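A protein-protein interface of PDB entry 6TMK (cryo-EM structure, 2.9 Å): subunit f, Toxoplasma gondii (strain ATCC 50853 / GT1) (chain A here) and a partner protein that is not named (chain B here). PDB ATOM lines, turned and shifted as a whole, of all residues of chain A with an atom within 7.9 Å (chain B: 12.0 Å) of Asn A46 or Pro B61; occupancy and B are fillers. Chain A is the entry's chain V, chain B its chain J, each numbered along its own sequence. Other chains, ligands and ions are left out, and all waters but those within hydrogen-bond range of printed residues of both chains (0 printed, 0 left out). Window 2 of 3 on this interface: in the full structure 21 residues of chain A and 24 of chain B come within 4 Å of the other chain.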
ATOM      1  N   PHE A   3      16.263  21.877   0.783  1.00  0.00           N
ATOM      2  CA  PHE A   3      15.632  20.727   0.155  1.00  0.00           C
ATOM      3  C   PHE A   3      16.607  20.114  -0.837  1.00  0.00           C
ATOM      4  O   PHE A   3      17.550  20.764  -1.292  1.00  0.00           O
ATOM      5  CB  PHE A   3      14.330  21.124  -0.544  1.00  0.00           C
ATOM      6  CG  PHE A   3      14.530  21.959  -1.766  1.00  0.00           C
ATOM      7  CD1 PHE A   3      14.953  23.262  -1.677  1.00  0.00           C
ATOM      8  CD2 PHE A   3      14.245  21.445  -3.009  1.00  0.00           C
ATOM      9  CE1 PHE A   3      15.129  24.018  -2.808  1.00  0.00           C
ATOM     10  CE2 PHE A   3      14.416  22.198  -4.138  1.00  0.00           C
ATOM     11  CZ  PHE A   3      14.855  23.489  -4.036  1.00  0.00           C
ATOM     12  N   TYR A   8      21.848  16.795  -4.071  1.00  0.00           N
ATOM     13  CA  TYR A   8      23.122  17.501  -4.029  1.00  0.00           C
ATOM     14  C   TYR A   8      24.285  16.530  -3.838  1.00  0.00           C
ATOM     15  O   TYR A   8      25.339  16.672  -4.476  1.00  0.00           O
ATOM     16  CB  TYR A   8      23.102  18.532  -2.907  1.00  0.00           C
ATOM     17  CG  TYR A   8      21.947  19.503  -2.963  1.00  0.00           C
ATOM     18  CD1 TYR A   8      21.325  19.811  -4.157  1.00  0.00           C
ATOM     19  CD2 TYR A   8      21.483  20.114  -1.814  1.00  0.00           C
ATOM     20  CE1 TYR A   8      20.270  20.686  -4.199  1.00  0.00           C
ATOM     21  CE2 TYR A   8      20.431  20.990  -1.849  1.00  0.00           C
ATOM     22  CZ  TYR A   8      19.831  21.274  -3.044  1.00  0.00           C
ATOM     23  OH  TYR A   8      18.778  22.149  -3.082  1.00  0.00           O
ATOM     24  N   ASP A  39      24.030  30.092 -16.188  1.00  0.00           N
ATOM     25  CA  ASP A  39      23.332  28.839 -15.930  1.00  0.00           C
ATOM     26  C   ASP A  39      23.414  28.466 -14.457  1.00  0.00           C
ATOM     27  O   ASP A  39      22.415  28.073 -13.842  1.00  0.00           O
ATOM     28  CB  ASP A  39      23.917  27.737 -16.804  1.00  0.00           C
ATOM     29  CG  ASP A  39      23.460  27.831 -18.243  1.00  0.00           C
ATOM     30  OD1 ASP A  39      23.839  26.954 -19.047  1.00  0.00           O
ATOM     31  OD2 ASP A  39      22.725  28.783 -18.573  1.00  0.00           O
ATOM     32  N   ALA A  40      24.607  28.580 -13.874  1.00  0.00           N
ATOM     33  CA  ALA A  40      24.769  28.245 -12.465  1.00  0.00           C
ATOM     34  C   ALA A  40      23.965  29.186 -11.576  1.00  0.00           C
ATOM     35  O   ALA A  40      23.309  28.752 -10.617  1.00  0.00           O
ATOM     36  CB  ALA A  40      26.246  28.289 -12.095  1.00  0.00           C
ATOM     37  N   LEU A  41      24.012  30.483 -11.877  1.00  0.00           N
ATOM     38  CA  LEU A  41      23.243  31.455 -11.112  1.00  0.00           C
ATOM     39  C   LEU A  41      21.752  31.176 -11.213  1.00  0.00           C
ATOM     40  O   LEU A  41      21.022  31.285 -10.222  1.00  0.00           O
ATOM     41  CB  LEU A  41      23.569  32.858 -11.606  1.00  0.00           C
ATOM     42  CG  LEU A  41      23.377  34.022 -10.645  1.00  0.00           C
ATOM     43  CD1 LEU A  41      24.342  33.929  -9.494  1.00  0.00           C
ATOM     44  CD2 LEU A  41      23.561  35.312 -11.393  1.00  0.00           C
ATOM     45  N   ALA A  42      21.284  30.805 -12.404  1.00  0.00           N
ATOM     46  CA  ALA A  42      19.878  30.482 -12.587  1.00  0.00           C
ATOM     47  C   ALA A  42      19.491  29.245 -11.792  1.00  0.00           C
ATOM     48  O   ALA A  42      18.396  29.185 -11.230  1.00  0.00           O
ATOM     49  CB  ALA A  42      19.588  30.288 -14.070  1.00  0.00           C
ATOM     50  N   TRP A  43      20.369  28.246 -11.745  1.00  0.00           N
ATOM     51  CA  TRP A  43      20.092  27.052 -10.954  1.00  0.00           C
ATOM     52  C   TRP A  43      19.942  27.400  -9.478  1.00  0.00           C
ATOM     53  O   TRP A  43      18.993  26.965  -8.808  1.00  0.00           O
ATOM     54  CB  TRP A  43      21.202  26.022 -11.166  1.00  0.00           C
ATOM     55  CG  TRP A  43      20.936  24.721 -10.500  1.00  0.00           C
ATOM     56  CD1 TRP A  43      20.179  23.704 -10.976  1.00  0.00           C
ATOM     57  CD2 TRP A  43      21.431  24.293  -9.230  1.00  0.00           C
ATOM     58  NE1 TRP A  43      20.161  22.669 -10.082  1.00  0.00           N
ATOM     59  CE2 TRP A  43      20.926  23.006  -9.000  1.00  0.00           C
ATOM     60  CE3 TRP A  43      22.251  24.875  -8.264  1.00  0.00           C
ATOM     61  CZ2 TRP A  43      21.209  22.293  -7.846  1.00  0.00           C
ATOM     62  CZ3 TRP A  43      22.528  24.168  -7.124  1.00  0.00           C
ATOM     63  CH2 TRP A  43      22.012  22.892  -6.923  1.00  0.00           C
ATOM     64  N   THR A  44      20.874  28.195  -8.954  1.00  0.00           N
ATOM     65  CA  THR A  44      20.802  28.577  -7.549  1.00  0.00           C
ATOM     66  C   THR A  44      19.540  29.383  -7.261  1.00  0.00           C
ATOM     67  O   THR A  44      18.873  29.176  -6.234  1.00  0.00           O
ATOM     68  CB  THR A  44      22.052  29.370  -7.172  1.00  0.00           C
ATOM     69  OG1 THR A  44      23.216  28.678  -7.632  1.00  0.00           O
ATOM     70  CG2 THR A  44      22.150  29.533  -5.682  1.00  0.00           C
ATOM     71  N   ASN A  45      19.199  30.313  -8.155  1.00  0.00           N
ATOM     72  CA  ASN A  45      17.969  31.075  -8.001  1.00  0.00           C
ATOM     73  C   ASN A  45      16.747  30.172  -8.025  1.00  0.00           C
ATOM     74  O   ASN A  45      15.796  30.394  -7.275  1.00  0.00           O
ATOM     75  CB  ASN A  45      17.857  32.133  -9.089  1.00  0.00           C
ATOM     76  CG  ASN A  45      16.661  33.027  -8.893  1.00  0.00           C
ATOM     77  OD1 ASN A  45      16.645  33.870  -8.003  1.00  0.00           O
ATOM     78  ND2 ASN A  45      15.640  32.832  -9.708  1.00  0.00           N
ATOM     79  N   ASN A  46      16.744  29.162  -8.890  1.00  0.00           N
ATOM     80  CA  ASN A  46      15.610  28.251  -8.955  1.00  0.00           C
ATOM     81  C   ASN A  46      15.447  27.503  -7.644  1.00  0.00           C
ATOM     82  O   ASN A  46      14.326  27.314  -7.162  1.00  0.00           O
ATOM     83  CB  ASN A  46      15.788  27.279 -10.118  1.00  0.00           C
ATOM     84  CG  ASN A  46      14.524  26.519 -10.443  1.00  0.00           C
ATOM     85  OD1 ASN A  46      13.428  27.072 -10.418  1.00  0.00           O
ATOM     86  ND2 ASN A  46      14.671  25.238 -10.755  1.00  0.00           N
ATOM     87  N   GLN A  47      16.557  27.100  -7.035  1.00  0.00           N
ATOM     88  CA  GLN A  47      16.479  26.427  -5.744  1.00  0.00           C
ATOM     89  C   GLN A  47      15.878  27.345  -4.685  1.00  0.00           C
ATOM     90  O   GLN A  47      14.911  26.984  -3.992  1.00  0.00           O
ATOM     91  CB  GLN A  47      17.867  25.964  -5.312  1.00  0.00           C
ATOM     92  CG  GLN A  47      18.520  24.959  -6.220  1.00  0.00           C
ATOM     93  CD  GLN A  47      17.794  23.642  -6.251  1.00  0.00           C
ATOM     94  OE1 GLN A  47      17.644  22.975  -5.230  1.00  0.00           O
ATOM     95  NE2 GLN A  47      17.354  23.246  -7.428  1.00  0.00           N
ATOM     96  N   PHE A  48      16.438  28.544  -4.547  1.00  0.00           N
ATOM     97  CA  PHE A  48      15.952  29.442  -3.506  1.00  0.00           C
ATOM     98  C   PHE A  48      14.519  29.889  -3.767  1.00  0.00           C
ATOM     99  O   PHE A  48      13.754  30.108  -2.820  1.00  0.00           O
ATOM    100  CB  PHE A  48      16.882  30.643  -3.385  1.00  0.00           C
ATOM    101  CG  PHE A  48      18.166  30.334  -2.686  1.00  0.00           C
ATOM    102  CD1 PHE A  48      18.186  30.033  -1.344  1.00  0.00           C
ATOM    103  CD2 PHE A  48      19.357  30.350  -3.376  1.00  0.00           C
ATOM    104  CE1 PHE A  48      19.367  29.746  -0.708  1.00  0.00           C
ATOM    105  CE2 PHE A  48      20.537  30.066  -2.744  1.00  0.00           C
ATOM    106  CZ  PHE A  48      20.544  29.765  -1.410  1.00  0.00           C
ATOM    107  N   ALA A  49      14.126  30.008  -5.035  1.00  0.00           N
ATOM    108  CA  ALA A  49      12.755  30.372  -5.364  1.00  0.00           C
ATOM    109  C   ALA A  49      11.788  29.236  -5.067  1.00  0.00           C
ATOM    110  O   ALA A  49      10.660  29.476  -4.622  1.00  0.00           O
ATOM    111  CB  ALA A  49      12.683  30.784  -6.829  1.00  0.00           C
ATOM    112  N   GLN A  50      12.204  27.990  -5.314  1.00  0.00           N
ATOM    113  CA  GLN A  50      11.398  26.857  -4.885  1.00  0.00           C
ATOM    114  C   GLN A  50      11.150  26.914  -3.392  1.00  0.00           C
ATOM    115  O   GLN A  50      10.029  26.688  -2.931  1.00  0.00           O
ATOM    116  CB  GLN A  50      12.091  25.542  -5.221  1.00  0.00           C
ATOM    117  CG  GLN A  50      12.000  25.077  -6.635  1.00  0.00           C
ATOM    118  CD  GLN A  50      12.821  23.830  -6.853  1.00  0.00           C
ATOM    119  OE1 GLN A  50      12.547  22.790  -6.267  1.00  0.00           O
ATOM    120  NE2 GLN A  50      13.842  23.931  -7.682  1.00  0.00           N
ATOM    121  N   ILE A  51      12.188  27.229  -2.620  1.00  0.00           N
ATOM    122  CA  ILE A  51      12.004  27.359  -1.177  1.00  0.00           C
ATOM    123  C   ILE A  51      10.992  28.454  -0.870  1.00  0.00           C
ATOM    124  O   ILE A  51      10.000  28.232  -0.163  1.00  0.00           O
ATOM    125  CB  ILE A  51      13.348  27.617  -0.477  1.00  0.00           C
ATOM    126  CG1 ILE A  51      14.269  26.419  -0.671  1.00  0.00           C
ATOM    127  CG2 ILE A  51      13.136  27.894   0.991  1.00  0.00           C
ATOM    128  CD1 ILE A  51      15.682  26.661  -0.259  1.00  0.00           C
ATOM    129  N   SER A  52      11.234  29.656  -1.391  1.00  0.00           N
ATOM    130  CA  SER A  52      10.393  30.797  -1.050  1.00  0.00           C
ATOM    131  C   SER A  52       8.936  30.551  -1.403  1.00  0.00           C
ATOM    132  O   SER A  52       8.041  31.007  -0.686  1.00  0.00           O
ATOM    133  CB  SER A  52      10.899  32.050  -1.759  1.00  0.00           C
ATOM    134  OG  SER A  52      12.254  32.310  -1.452  1.00  0.00           O
ATOM    135  N   ARG A  53       8.674  29.834  -2.494  1.00  0.00           N
ATOM    136  CA  ARG A  53       7.298  29.560  -2.883  1.00  0.00           C
ATOM    137  C   ARG A  53       6.689  28.430  -2.061  1.00  0.00           C
ATOM    138  O   ARG A  53       5.590  28.575  -1.518  1.00  0.00           O
ATOM    139  CB  ARG A  53       7.256  29.232  -4.372  1.00  0.00           C
ATOM    140  CG  ARG A  53       5.903  28.850  -4.919  1.00  0.00           C
ATOM    141  CD  ARG A  53       4.842  29.867  -4.619  1.00  0.00           C
ATOM    142  NE  ARG A  53       3.621  29.555  -5.347  1.00  0.00           N
ATOM    143  CZ  ARG A  53       2.420  29.409  -4.799  1.00  0.00           C
ATOM    144  NH1 ARG A  53       1.384  29.125  -5.568  1.00  0.00           N
ATOM    145  NH2 ARG A  53       2.238  29.552  -3.499  1.00  0.00           N
ATOM    146  N   PRO B  54       8.996  21.279 -21.519  1.00  0.00           N
ATOM    147  CA  PRO B  54       9.566  21.522 -20.195  1.00  0.00           C
ATOM    148  C   PRO B  54       8.721  22.498 -19.399  1.00  0.00           C
ATOM    149  O   PRO B  54       7.880  23.225 -19.931  1.00  0.00           O
ATOM    150  CB  PRO B  54      10.948  22.112 -20.500  1.00  0.00           C
ATOM    151  CG  PRO B  54      11.165  21.897 -21.952  1.00  0.00           C
ATOM    152  CD  PRO B  54       9.816  21.902 -22.564  1.00  0.00           C
ATOM    153  N   MET B  55       8.965  22.505 -18.092  1.00  0.00           N
ATOM    154  CA  MET B  55       8.227  23.381 -17.202  1.00  0.00           C
ATOM    155  C   MET B  55       8.771  24.799 -17.194  1.00  0.00           C
ATOM    156  O   MET B  55       8.077  25.709 -16.736  1.00  0.00           O
ATOM    157  CB  MET B  55       8.245  22.812 -15.788  1.00  0.00           C
ATOM    158  CG  MET B  55       7.370  23.547 -14.804  1.00  0.00           C
ATOM    159  SD  MET B  55       5.640  23.527 -15.273  1.00  0.00           S
ATOM    160  CE  MET B  55       5.187  21.950 -14.581  1.00  0.00           C
ATOM    161  N   LYS B  56       9.998  25.013 -17.670  1.00  0.00           N
ATOM    162  CA  LYS B  56      10.526  26.368 -17.724  1.00  0.00           C
ATOM    163  C   LYS B  56       9.857  27.199 -18.807  1.00  0.00           C
ATOM    164  O   LYS B  56       9.920  28.430 -18.753  1.00  0.00           O
ATOM    165  CB  LYS B  56      12.035  26.338 -17.945  1.00  0.00           C
ATOM    166  CG  LYS B  56      12.469  25.784 -19.273  1.00  0.00           C
ATOM    167  CD  LYS B  56      13.974  25.647 -19.343  1.00  0.00           C
ATOM    168  CE  LYS B  56      14.406  24.880 -20.578  1.00  0.00           C
ATOM    169  NZ  LYS B  56      15.881  24.925 -20.795  1.00  0.00           N
ATOM    170  N   GLU B  57       9.225  26.559 -19.788  1.00  0.00           N
ATOM    171  CA  GLU B  57       8.435  27.279 -20.773  1.00  0.00           C
ATOM    172  C   GLU B  57       7.093  27.744 -20.228  1.00  0.00           C
ATOM    173  O   GLU B  57       6.374  28.461 -20.928  1.00  0.00           O
ATOM    174  CB  GLU B  57       8.202  26.400 -22.000  1.00  0.00           C
ATOM    175  CG  GLU B  57       9.469  25.969 -22.699  1.00  0.00           C
ATOM    176  CD  GLU B  57       9.195  25.258 -24.006  1.00  0.00           C
ATOM    177  OE1 GLU B  57       8.008  25.074 -24.344  1.00  0.00           O
ATOM    178  OE2 GLU B  57      10.166  24.882 -24.696  1.00  0.00           O
ATOM    179  N   ILE B  58       6.739  27.354 -19.006  1.00  0.00           N
ATOM    180  CA  ILE B  58       5.413  27.615 -18.467  1.00  0.00           C
ATOM    181  C   ILE B  58       5.540  28.423 -17.187  1.00  0.00           C
ATOM    182  O   ILE B  58       5.013  29.535 -17.081  1.00  0.00           O
ATOM    183  CB  ILE B  58       4.658  26.303 -18.210  1.00  0.00           C
ATOM    184  CG1 ILE B  58       4.422  25.561 -19.516  1.00  0.00           C
ATOM    185  CG2 ILE B  58       3.336  26.586 -17.565  1.00  0.00           C
ATOM    186  CD1 ILE B  58       4.374  24.089 -19.361  1.00  0.00           C
ATOM    187  N   LEU B  59       6.234  27.859 -16.205  1.00  0.00           N
ATOM    188  CA  LEU B  59       6.420  28.483 -14.905  1.00  0.00           C
ATOM    189  C   LEU B  59       7.801  29.123 -14.871  1.00  0.00           C
ATOM    190  O   LEU B  59       8.816  28.425 -14.922  1.00  0.00           O
ATOM    191  CB  LEU B  59       6.276  27.453 -13.790  1.00  0.00           C
ATOM    192  CG  LEU B  59       4.967  26.676 -13.710  1.00  0.00           C
ATOM    193  CD1 LEU B  59       5.031  25.668 -12.594  1.00  0.00           C
ATOM    194  CD2 LEU B  59       3.800  27.605 -13.500  1.00  0.00           C
ATOM    195  N   GLN B  60       7.834  30.436 -14.786  1.00  0.00           N
ATOM    196  CA  GLN B  60       9.085  31.166 -14.684  1.00  0.00           C
ATOM    197  C   GLN B  60       9.389  31.451 -13.227  1.00  0.00           C
ATOM    198  O   GLN B  60       8.519  31.970 -12.516  1.00  0.00           O
ATOM    199  CB  GLN B  60       9.009  32.475 -15.462  1.00  0.00           C
ATOM    200  CG  GLN B  60       8.611  32.314 -16.907  1.00  0.00           C
ATOM    201  CD  GLN B  60       9.655  31.594 -17.724  1.00  0.00           C
ATOM    202  OE1 GLN B  60      10.855  31.759 -17.506  1.00  0.00           O
ATOM    203  NE2 GLN B  60       9.205  30.790 -18.676  1.00  0.00           N
ATOM    204  N   PRO B  61      10.579  31.139 -12.728  1.00  0.00           N
ATOM    205  CA  PRO B  61      10.892  31.470 -11.341  1.00  0.00           C
ATOM    206  C   PRO B  61      11.277  32.927 -11.170  1.00  0.00           C
ATOM    207  O   PRO B  61      11.869  33.557 -12.047  1.00  0.00           O
ATOM    208  CB  PRO B  61      12.074  30.550 -11.025  1.00  0.00           C
ATOM    209  CG  PRO B  61      12.729  30.366 -12.303  1.00  0.00           C
ATOM    210  CD  PRO B  61      11.663  30.359 -13.344  1.00  0.00           C
ATOM    211  N   LEU B  62      10.916  33.459 -10.011  1.00  0.00           N
ATOM    212  CA  LEU B  62      11.318  34.801  -9.650  1.00  0.00           C
ATOM    213  C   LEU B  62      12.818  34.861  -9.393  1.00  0.00           C
ATOM    214  O   LEU B  62      13.469  33.859  -9.090  1.00  0.00           O
ATOM    215  CB  LEU B  62      10.570  35.267  -8.406  1.00  0.00           C
ATOM    216  CG  LEU B  62       9.082  35.552  -8.529  1.00  0.00           C
ATOM    217  CD1 LEU B  62       8.534  35.745  -7.159  1.00  0.00           C
ATOM    218  CD2 LEU B  62       8.824  36.788  -9.362  1.00  0.00           C
ATOM    219  N   TRP B  63      13.364  36.063  -9.520  1.00  0.00           N
ATOM    220  CA  TRP B  63      14.768  36.311  -9.238  1.00  0.00           C
ATOM    221  C   TRP B  63      14.904  36.744  -7.786  1.00  0.00           C
ATOM    222  O   TRP B  63      14.354  37.775  -7.385  1.00  0.00           O
ATOM    223  CB  TRP B  63      15.341  37.369 -10.175  1.00  0.00           C
ATOM    224  CG  TRP B  63      16.793  37.220 -10.411  1.00  0.00           C
ATOM    225  CD1 TRP B  63      17.770  38.036  -9.944  1.00  0.00           C
ATOM    226  CD2 TRP B  63      17.451  36.192 -11.155  1.00  0.00           C
ATOM    227  NE1 TRP B  63      18.997  37.588 -10.349  1.00  0.00           N
ATOM    228  CE2 TRP B  63      18.828  36.455 -11.097  1.00  0.00           C
ATOM    229  CE3 TRP B  63      17.010  35.078 -11.869  1.00  0.00           C
ATOM    230  CZ2 TRP B  63      19.766  35.649 -11.719  1.00  0.00           C
ATOM    231  CZ3 TRP B  63      17.945  34.279 -12.486  1.00  0.00           C
ATOM    232  CH2 TRP B  63      19.305  34.568 -12.408  1.00  0.00           C
ATOM    233  N   VAL B  64      15.627  35.947  -6.996  1.00  0.00           N
ATOM    234  CA  VAL B  64      15.765  36.187  -5.568  1.00  0.00           C
ATOM    235  C   VAL B  64      17.207  36.099  -5.096  1.00  0.00           C
ATOM    236  O   VAL B  64      17.477  36.361  -3.925  1.00  0.00           O
ATOM    237  CB  VAL B  64      14.879  35.222  -4.754  1.00  0.00           C
ATOM    238  CG1 VAL B  64      13.446  35.322  -5.199  1.00  0.00           C
ATOM    239  CG2 VAL B  64      15.348  33.804  -4.894  1.00  0.00           C
ATOM    240  N   VAL B  65      18.148  35.750  -5.974  1.00  0.00           N
ATOM    241  CA  VAL B  65      19.531  35.575  -5.548  1.00  0.00           C
ATOM    242  C   VAL B  65      20.146  36.917  -5.195  1.00  0.00           C
ATOM    243  O   VAL B  65      20.862  37.049  -4.196  1.00  0.00           O
ATOM    244  CB  VAL B  65      20.339  34.853  -6.638  1.00  0.00           C
ATOM    245  CG1 VAL B  65      21.797  34.838  -6.286  1.00  0.00           C
ATOM    246  CG2 VAL B  65      19.857  33.459  -6.764  1.00  0.00           C
ATOM    247  N   GLU B  66      19.890  37.924  -6.016  1.00  0.00           N
ATOM    248  CA  GLU B  66      20.343  39.273  -5.777  1.00  0.00           C
ATOM    249  C   GLU B  66      19.136  40.139  -5.483  1.00  0.00           C
ATOM    250  O   GLU B  66      18.139  40.058  -6.210  1.00  0.00           O
ATOM    251  CB  GLU B  66      21.106  39.817  -6.985  1.00  0.00           C
ATOM    252  CG  GLU B  66      20.307  39.872  -8.255  1.00  0.00           C
ATOM    253  CD  GLU B  66      21.179  39.860  -9.491  1.00  0.00           C
ATOM    254  OE1 GLU B  66      22.071  38.992  -9.582  1.00  0.00           O
ATOM    255  OE2 GLU B  66      20.973  40.716 -10.376  1.00  0.00           O
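Leu A41 touches Trp B63 (CD2 to CZ2, 3.8 Å).
CA of Trp B63 touches OD1 of Asn A45, 3.3 Å away.
Asn A46 touches Pro B61 (OD1 to CB, 3.8 Å).
Val B64 touches Phe A48 (CG2 to CB, 3.8 Å).
Ala A49 touches Leu B62 (CB to O, 3.9 Å).
Val B64 touches Ala A49.
Of the 13 printed residues of chain B, 5 touch a printed residue of chain A.
Printed residues of chain B that touch a printed residue of chain A: Pro B61, Leu B62, Trp B63, Val B64 and Val B65.
Hydrophobic or aromatic side chains of chain B within 4 Å of the printed part of chain A: Pro B61, Trp B63, Val B64 and Val B65.
Of the 17 printed residues of chain A, 5 touch a printed residue of chain B.
Printed residues of chain A that touch a printed residue of chain B: Leu A41, Asn A45, Asn A46, Phe A48 and Ala A49.
Hydrophobic or aromatic side chains of chain A that line the printed part of chain B: Leu A41, Phe A48 and Ala A49.
Among the printed residues, no Asp or Glu carboxylate lies within 4 Å of a Lys or Arg side-chain nitrogen of the other chain.
Asn A46 touches just one residue of chain B: Pro B61 (3.8 Å).
No residue of chain B comes within 4 Å of Thr A44.
Asn A45 touches just these residues of chain B: Leu B62, Trp B63, Val B64 and Val B65.
No residue of chain B comes within 4 Å of Gln A47.
Of the printed residues of chain B, Leu A41 touches Trp B63 (3.8 Å).
Of the printed residues of chain A, Leu B62 touches Asn A45 (2.5 Å) and Ala A49 (3.9 Å).
Of the printed residues of chain A, Val B65 touches Asn A45.
Of the printed residues of chain A, Val B64 touches Asn A45, Phe A48 and Ala A49.
Trp A43 touches none of the printed residues of chain B.
The nearest residue of chain A that does not touch Pro B61 is Ala A49 (4.2 Å).
The backbone carbonyl oxygen (O) of Leu B62 is in hydrogen-bond range of the side-chain amide nitrogen (ND2) of Asn A45 (2.5 Å).
The side-chain amide oxygen (OD1) of Asn A45 is in hydrogen-bond range of the backbone NH (N) of Val B64 (2.5 Å).
OD1 of Asn A45 sits at hydrogen-bond distance from N of Val B65.
ND2 of Asn A46 sits close to NE2 of Gln A50, at 3.4 Å.
OG of Ser A52 is in hydrogen-bond range of O of Phe A48.
OE1 of Glu B66 lies close to NE1 of Trp B63, 3.5 Å away.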
